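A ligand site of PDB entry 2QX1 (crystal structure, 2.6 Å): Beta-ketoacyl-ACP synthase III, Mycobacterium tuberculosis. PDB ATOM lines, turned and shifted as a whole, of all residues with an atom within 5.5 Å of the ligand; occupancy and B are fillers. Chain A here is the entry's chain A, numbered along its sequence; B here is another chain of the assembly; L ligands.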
ATOM      1  N   ASN A  91      31.831  26.638  25.837  1.00  0.00           N
ATOM      2  CA  ASN A  91      31.564  25.365  25.152  1.00  0.00           C
ATOM      3  C   ASN A  91      30.677  25.544  23.912  1.00  0.00           C
ATOM      4  O   ASN A  91      30.266  24.576  23.293  1.00  0.00           O
ATOM      5  CB  ASN A  91      30.869  24.388  26.103  1.00  0.00           C
ATOM      6  CG  ASN A  91      31.348  24.525  27.516  1.00  0.00           C
ATOM      7  OD1 ASN A  91      32.400  23.990  27.877  1.00  0.00           O
ATOM      8  ND2 ASN A  91      30.587  25.234  28.341  1.00  0.00           N
ATOM      9  N   THR A  92      30.359  26.786  23.556  1.00  0.00           N
ATOM     10  CA  THR A  92      29.495  27.026  22.394  1.00  0.00           C
ATOM     11  C   THR A  92      30.105  27.947  21.321  1.00  0.00           C
ATOM     12  O   THR A  92      29.414  28.733  20.688  1.00  0.00           O
ATOM     13  CB  THR A  92      28.045  27.449  22.786  1.00  0.00           C
ATOM     14  OG1 THR A  92      28.077  28.519  23.738  1.00  0.00           O
ATOM     15  CG2 THR A  92      27.281  26.276  23.378  1.00  0.00           C
ATOM     16  N   GLY A 121      34.003  22.192  30.208  1.00  0.00           N
ATOM     17  CA  GLY A 121      32.578  22.043  30.483  1.00  0.00           C
ATOM     18  C   GLY A 121      32.039  23.242  31.248  1.00  0.00           C
ATOM     19  O   GLY A 121      32.459  24.370  30.999  1.00  0.00           O
ATOM     20  N   CYS A 122      31.153  22.995  32.203  1.00  0.00           N
ATOM     21  CA  CYS A 122      30.598  24.073  32.999  1.00  0.00           C
ATOM     22  C   CYS A 122      31.634  24.762  33.905  1.00  0.00           C
ATOM     23  O   CYS A 122      31.626  25.986  34.044  1.00  0.00           O
ATOM     24  CB  CYS A 122      29.369  23.610  33.782  1.00  0.00           C
ATOM     25  SG  CYS A 122      27.889  23.317  32.755  1.00  0.00           S
ATOM     26  N   GLU A 150      28.317  31.960  26.543  1.00  0.00           N
ATOM     27  CA  GLU A 150      27.633  30.761  26.092  1.00  0.00           C
ATOM     28  C   GLU A 150      26.356  31.024  25.249  1.00  0.00           C
ATOM     29  O   GLU A 150      25.477  31.776  25.663  1.00  0.00           O
ATOM     30  CB  GLU A 150      27.312  29.880  27.314  1.00  0.00           C
ATOM     31  CG  GLU A 150      27.487  28.386  27.066  1.00  0.00           C
ATOM     32  CD  GLU A 150      28.928  27.905  27.173  1.00  0.00           C
ATOM     33  OE1 GLU A 150      29.489  27.991  28.290  1.00  0.00           O
ATOM     34  OE2 GLU A 150      29.492  27.430  26.156  1.00  0.00           O
ATOM     35  N   LEU A 152      23.918  28.442  24.006  1.00  0.00           N
ATOM     36  CA  LEU A 152      23.464  27.058  24.019  1.00  0.00           C
ATOM     37  C   LEU A 152      22.151  26.798  23.267  1.00  0.00           C
ATOM     38  O   LEU A 152      21.883  25.660  22.881  1.00  0.00           O
ATOM     39  CB  LEU A 152      23.353  26.598  25.471  1.00  0.00           C
ATOM     40  CG  LEU A 152      24.685  26.486  26.215  1.00  0.00           C
ATOM     41  CD1 LEU A 152      24.673  27.243  27.517  1.00  0.00           C
ATOM     42  CD2 LEU A 152      24.986  25.045  26.463  1.00  0.00           C
ATOM     43  N   THR A 155      21.999  24.247  20.512  1.00  0.00           N
ATOM     44  CA  THR A 155      22.360  22.879  20.913  1.00  0.00           C
ATOM     45  C   THR A 155      21.206  22.149  21.610  1.00  0.00           C
ATOM     46  O   THR A 155      21.332  20.956  21.932  1.00  0.00           O
ATOM     47  CB  THR A 155      23.620  22.819  21.832  1.00  0.00           C
ATOM     48  OG1 THR A 155      23.282  23.314  23.132  1.00  0.00           O
ATOM     49  CG2 THR A 155      24.806  23.617  21.266  1.00  0.00           C
ATOM     50  N   PHE A 167      19.160  24.804  29.657  1.00  0.00           N
ATOM     51  CA  PHE A 167      20.219  25.638  29.124  1.00  0.00           C
ATOM     52  C   PHE A 167      19.747  26.980  28.570  1.00  0.00           C
ATOM     53  O   PHE A 167      18.670  27.077  27.995  1.00  0.00           O
ATOM     54  CB  PHE A 167      21.015  24.859  28.075  1.00  0.00           C
ATOM     55  CG  PHE A 167      21.763  23.663  28.633  1.00  0.00           C
ATOM     56  CD1 PHE A 167      21.256  22.382  28.477  1.00  0.00           C
ATOM     57  CD2 PHE A 167      22.965  23.832  29.318  1.00  0.00           C
ATOM     58  CE1 PHE A 167      21.941  21.288  28.988  1.00  0.00           C
ATOM     59  CE2 PHE A 167      23.660  22.743  29.837  1.00  0.00           C
ATOM     60  CZ  PHE A 167      23.148  21.471  29.673  1.00  0.00           C
ATOM     61  N   ILE A 199      27.012  14.710  30.691  1.00  0.00           N
ATOM     62  CA  ILE A 199      26.663  15.907  29.939  1.00  0.00           C
ATOM     63  C   ILE A 199      27.511  15.881  28.662  1.00  0.00           C
ATOM     64  O   ILE A 199      28.735  15.891  28.727  1.00  0.00           O
ATOM     65  CB  ILE A 199      26.929  17.199  30.739  1.00  0.00           C
ATOM     66  CG1 ILE A 199      26.406  17.058  32.180  1.00  0.00           C
ATOM     67  CG2 ILE A 199      26.334  18.412  29.995  1.00  0.00           C
ATOM     68  CD1 ILE A 199      26.666  18.243  33.113  1.00  0.00           C
ATOM     69  N   ARG A 200      26.851  15.835  27.511  1.00  0.00           N
ATOM     70  CA  ARG A 200      27.565  15.594  26.263  1.00  0.00           C
ATOM     71  C   ARG A 200      26.912  16.126  24.995  1.00  0.00           C
ATOM     72  O   ARG A 200      25.726  16.485  24.965  1.00  0.00           O
ATOM     73  CB  ARG A 200      27.809  14.101  26.081  1.00  0.00           C
ATOM     74  CG  ARG A 200      26.553  13.309  25.719  1.00  0.00           C
ATOM     75  CD  ARG A 200      26.841  11.823  25.795  1.00  0.00           C
ATOM     76  NE  ARG A 200      25.754  11.027  25.239  1.00  0.00           N
ATOM     77  CZ  ARG A 200      24.697  10.615  25.931  1.00  0.00           C
ATOM     78  NH1 ARG A 200      24.594  10.924  27.217  1.00  0.00           N
ATOM     79  NH2 ARG A 200      23.756   9.903  25.341  1.00  0.00           N
ATOM     80  N   GLN A 201      27.725  16.178  23.949  1.00  0.00           N
ATOM     81  CA  GLN A 201      27.253  16.205  22.593  1.00  0.00           C
ATOM     82  C   GLN A 201      27.164  14.738  22.224  1.00  0.00           C
ATOM     83  O   GLN A 201      28.127  13.981  22.434  1.00  0.00           O
ATOM     84  CB  GLN A 201      28.253  16.945  21.707  1.00  0.00           C
ATOM     85  CG  GLN A 201      27.852  17.041  20.250  1.00  0.00           C
ATOM     86  CD  GLN A 201      28.703  18.000  19.468  1.00  0.00           C
ATOM     87  OE1 GLN A 201      29.114  19.048  19.983  1.00  0.00           O
ATOM     88  NE2 GLN A 201      28.957  17.677  18.211  1.00  0.00           N
ATOM     89  N   TRP A 205      31.011  16.169  15.497  1.00  0.00           N
ATOM     90  CA  TRP A 205      30.722  16.876  14.264  1.00  0.00           C
ATOM     91  C   TRP A 205      31.198  16.170  13.003  1.00  0.00           C
ATOM     92  O   TRP A 205      30.528  16.250  11.968  1.00  0.00           O
ATOM     93  CB  TRP A 205      31.327  18.263  14.306  1.00  0.00           C
ATOM     94  CG  TRP A 205      30.734  19.136  15.319  1.00  0.00           C
ATOM     95  CD1 TRP A 205      31.340  19.595  16.451  1.00  0.00           C
ATOM     96  CD2 TRP A 205      29.408  19.663  15.328  1.00  0.00           C
ATOM     97  NE1 TRP A 205      30.474  20.389  17.162  1.00  0.00           N
ATOM     98  CE2 TRP A 205      29.275  20.443  16.498  1.00  0.00           C
ATOM     99  CE3 TRP A 205      28.318  19.555  14.458  1.00  0.00           C
ATOM    100  CZ2 TRP A 205      28.094  21.124  16.815  1.00  0.00           C
ATOM    101  CZ3 TRP A 205      27.137  20.235  14.774  1.00  0.00           C
ATOM    102  CH2 TRP A 205      27.044  21.002  15.941  1.00  0.00           C
ATOM    103  N   PRO A 217      23.566  16.656  15.885  1.00  0.00           N
ATOM    104  CA  PRO A 217      23.831  16.628  17.326  1.00  0.00           C
ATOM    105  C   PRO A 217      23.084  17.698  18.138  1.00  0.00           C
ATOM    106  O   PRO A 217      22.774  18.784  17.640  1.00  0.00           O
ATOM    107  CB  PRO A 217      25.355  16.835  17.410  1.00  0.00           C
ATOM    108  CG  PRO A 217      25.844  16.742  16.007  1.00  0.00           C
ATOM    109  CD  PRO A 217      24.714  17.171  15.144  1.00  0.00           C
ATOM    110  N   PHE A 218      22.792  17.338  19.377  1.00  0.00           N
ATOM    111  CA  PHE A 218      22.201  18.225  20.360  1.00  0.00           C
ATOM    112  C   PHE A 218      22.927  17.946  21.669  1.00  0.00           C
ATOM    113  O   PHE A 218      23.771  17.040  21.730  1.00  0.00           O
ATOM    114  CB  PHE A 218      20.710  17.931  20.534  1.00  0.00           C
ATOM    115  CG  PHE A 218      19.864  18.261  19.331  1.00  0.00           C
ATOM    116  CD1 PHE A 218      19.668  19.572  18.930  1.00  0.00           C
ATOM    117  CD2 PHE A 218      19.223  17.242  18.614  1.00  0.00           C
ATOM    118  CE1 PHE A 218      18.869  19.867  17.836  1.00  0.00           C
ATOM    119  CE2 PHE A 218      18.427  17.543  17.513  1.00  0.00           C
ATOM    120  CZ  PHE A 218      18.251  18.855  17.124  1.00  0.00           C
ATOM    121  N   VAL A 219      22.646  18.736  22.711  1.00  0.00           N
ATOM    122  CA  VAL A 219      23.205  18.463  24.047  1.00  0.00           C
ATOM    123  C   VAL A 219      22.388  17.401  24.775  1.00  0.00           C
ATOM    124  O   VAL A 219      21.153  17.411  24.734  1.00  0.00           O
ATOM    125  CB  VAL A 219      23.372  19.760  24.896  1.00  0.00           C
ATOM    126  CG1 VAL A 219      22.063  20.209  25.529  1.00  0.00           C
ATOM    127  CG2 VAL A 219      24.469  19.579  25.951  1.00  0.00           C
ATOM    128  N   HIS A 258      27.807  27.080  40.811  1.00  0.00           N
ATOM    129  CA  HIS A 258      27.356  27.032  39.445  1.00  0.00           C
ATOM    130  C   HIS A 258      25.852  26.781  39.393  1.00  0.00           C
ATOM    131  O   HIS A 258      25.312  25.940  40.131  1.00  0.00           O
ATOM    132  CB  HIS A 258      28.084  25.940  38.675  1.00  0.00           C
ATOM    133  CG  HIS A 258      27.494  25.693  37.336  1.00  0.00           C
ATOM    134  ND1 HIS A 258      27.756  26.501  36.246  1.00  0.00           N
ATOM    135  CD2 HIS A 258      26.608  24.758  36.912  1.00  0.00           C
ATOM    136  CE1 HIS A 258      27.077  26.053  35.199  1.00  0.00           C
ATOM    137  NE2 HIS A 258      26.377  25.002  35.574  1.00  0.00           N
ATOM    138  N   SER A 291      26.090  27.503  31.689  1.00  0.00           N
ATOM    139  CA  SER A 291      27.377  26.820  31.753  1.00  0.00           C
ATOM    140  C   SER A 291      28.537  27.737  32.226  1.00  0.00           C
ATOM    141  O   SER A 291      28.500  28.244  33.345  1.00  0.00           O
ATOM    142  CB  SER A 291      27.677  26.142  30.406  1.00  0.00           C
ATOM    143  OG  SER A 291      28.588  25.058  30.566  1.00  0.00           O
ATOM    144  N   TYR A 319      30.671  23.360  38.367  1.00  0.00           N
ATOM    145  CA  TYR A 319      30.501  21.944  38.040  1.00  0.00           C
ATOM    146  C   TYR A 319      29.643  21.724  36.804  1.00  0.00           C
ATOM    147  O   TYR A 319      28.709  22.484  36.527  1.00  0.00           O
ATOM    148  CB  TYR A 319      29.967  21.151  39.234  1.00  0.00           C
ATOM    149  CG  TYR A 319      28.625  21.608  39.756  1.00  0.00           C
ATOM    150  CD1 TYR A 319      27.436  21.000  39.332  1.00  0.00           C
ATOM    151  CD2 TYR A 319      28.551  22.638  40.688  1.00  0.00           C
ATOM    152  CE1 TYR A 319      26.217  21.415  39.828  1.00  0.00           C
ATOM    153  CE2 TYR A 319      27.327  23.069  41.181  1.00  0.00           C
ATOM    154  CZ  TYR A 319      26.164  22.467  40.748  1.00  0.00           C
ATOM    155  OH  TYR A 319      24.970  22.904  41.262  1.00  0.00           O
ATOM    156  N   GLY A 320      29.964  20.667  36.055  1.00  0.00           N
ATOM    157  CA  GLY A 320      29.302  20.403  34.803  1.00  0.00           C
ATOM    158  C   GLY A 320      30.051  19.420  33.925  1.00  0.00           C
ATOM    159  O   GLY A 320      30.661  18.486  34.431  1.00  0.00           O
ATOM    160  N   ALA A 321      30.012  19.674  32.614  1.00  0.00           N
ATOM    161  CA  ALA A 321      30.399  18.655  31.621  1.00  0.00           C
ATOM    162  C   ALA A 321      31.852  18.139  31.720  1.00  0.00           C
ATOM    163  O   ALA A 321      32.704  18.756  32.366  1.00  0.00           O
ATOM    164  CB  ALA A 321      30.075  19.123  30.222  1.00  0.00           C
ATOM    165  N   GLN B  96      31.680  19.807  21.272  1.00  0.00           N
ATOM    166  CA  GLN B  96      31.578  21.073  21.991  1.00  0.00           C
ATOM    167  C   GLN B  96      31.826  20.827  23.465  1.00  0.00           C
ATOM    168  O   GLN B  96      32.475  21.633  24.133  1.00  0.00           O
ATOM    169  CB  GLN B  96      30.199  21.718  21.814  1.00  0.00           C
ATOM    170  CG  GLN B  96      29.883  22.370  20.450  1.00  0.00           C
ATOM    171  CD  GLN B  96      31.082  23.072  19.795  1.00  0.00           C
ATOM    172  OE1 GLN B  96      31.453  22.720  18.677  1.00  0.00           O
ATOM    173  NE2 GLN B  96      31.690  24.042  20.494  1.00  0.00           N
ATOM    174  N   THR B  97      31.283  19.718  23.961  1.00  0.00           N
ATOM    175  CA  THR B  97      31.540  19.205  25.313  1.00  0.00           C
ATOM    176  C   THR B  97      31.247  17.717  25.198  1.00  0.00           C
ATOM    177  O   THR B  97      30.560  17.320  24.246  1.00  0.00           O
ATOM    178  CB  THR B  97      30.614  19.879  26.388  1.00  0.00           C
ATOM    179  OG1 THR B  97      31.293  19.936  27.643  1.00  0.00           O
ATOM    180  CG2 THR B  97      29.307  19.111  26.543  1.00  0.00           C
HETATM  181  C1  LIG L   1      25.623  19.952  20.692  1.00  0.00           C
HETATM  182  C2  LIG L   1      25.882  19.995  22.205  1.00  0.00           C
HETATM  183  C3  LIG L   1      27.363  20.252  22.477  1.00  0.00           C
HETATM  184  C4  LIG L   1      27.616  20.780  23.886  1.00  0.00           C
HETATM  185  C5  LIG L   1      27.365  22.288  23.947  1.00  0.00           C
HETATM  186  C6  LIG L   1      26.718  22.657  25.270  1.00  0.00           C
HETATM  187  C7  LIG L   1      27.727  22.673  26.416  1.00  0.00           C
HETATM  188  C8  LIG L   1      27.311  21.694  27.503  1.00  0.00           C
HETATM  189  C9  LIG L   1      28.105  21.945  28.772  1.00  0.00           C
HETATM  190  C10 LIG L   1      27.156  21.936  29.979  1.00  0.00           C
HETATM  191  S1  LIG L   1      28.031  21.703  31.565  1.00  0.00           S
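N of Cys 122 lies close to S1 of the ligand, at 3.4 Å. A sulfur (S1) of the ligand is bonded to the side-chain sulfur (SG) of Cys 122, at 2.0 Å. S1 of the ligand sits close to N of Ala 321. A sulfur (S1) of the ligand lies close to the side-chain hydroxyl (OG) of Ser 291 (3.5 Å).
A ring nitrogen (NE2) of His 258 sits at hydrogen-bond distance from the side-chain sulfur (SG) of Cys 122 (3.6 Å). The side-chain amide oxygen (OE1) of Gln 201 lies within hydrogen-bond range of the backbone NH (N) of Gln 96 of chain B (3.0 Å). The backbone NH of Asn 91 sits at hydrogen-bond distance from the side-chain carboxylate of Glu 150 (2.5 Å). ND2 of Asn 91 lies within hydrogen-bond range of OG of Ser 291, 3.0 Å away. O of Leu 152 is in hydrogen-bond range of OG1 of Thr 155. The side-chain amide oxygen (OD1) of Asn 91 sits close to the backbone carbonyl oxygen (O) of Gly 121 (3.1 Å). The side-chain amide nitrogen of Gln 96 of chain B sits at hydrogen-bond distance from the backbone carbonyl oxygen of Asn 91, 3.2 Å away. The side-chain hydroxyl (OG) of Ser 291 lies within hydrogen-bond range of the side-chain sulfur (SG) of Cys 122 (2.9 Å).
Residues that only touch the ligand: Asn 91, Leu 152, Thr 155, Phe 167, Ile 199, Gln 201, Phe 218, Val 219, Gly 320, Gln 96 of chain B and Thr 97 of chain B. Hydrophobic or aromatic side chains within 4 Å of the ligand: Leu 152, Phe 167, Ile 199, Val 219 and Ala 321.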
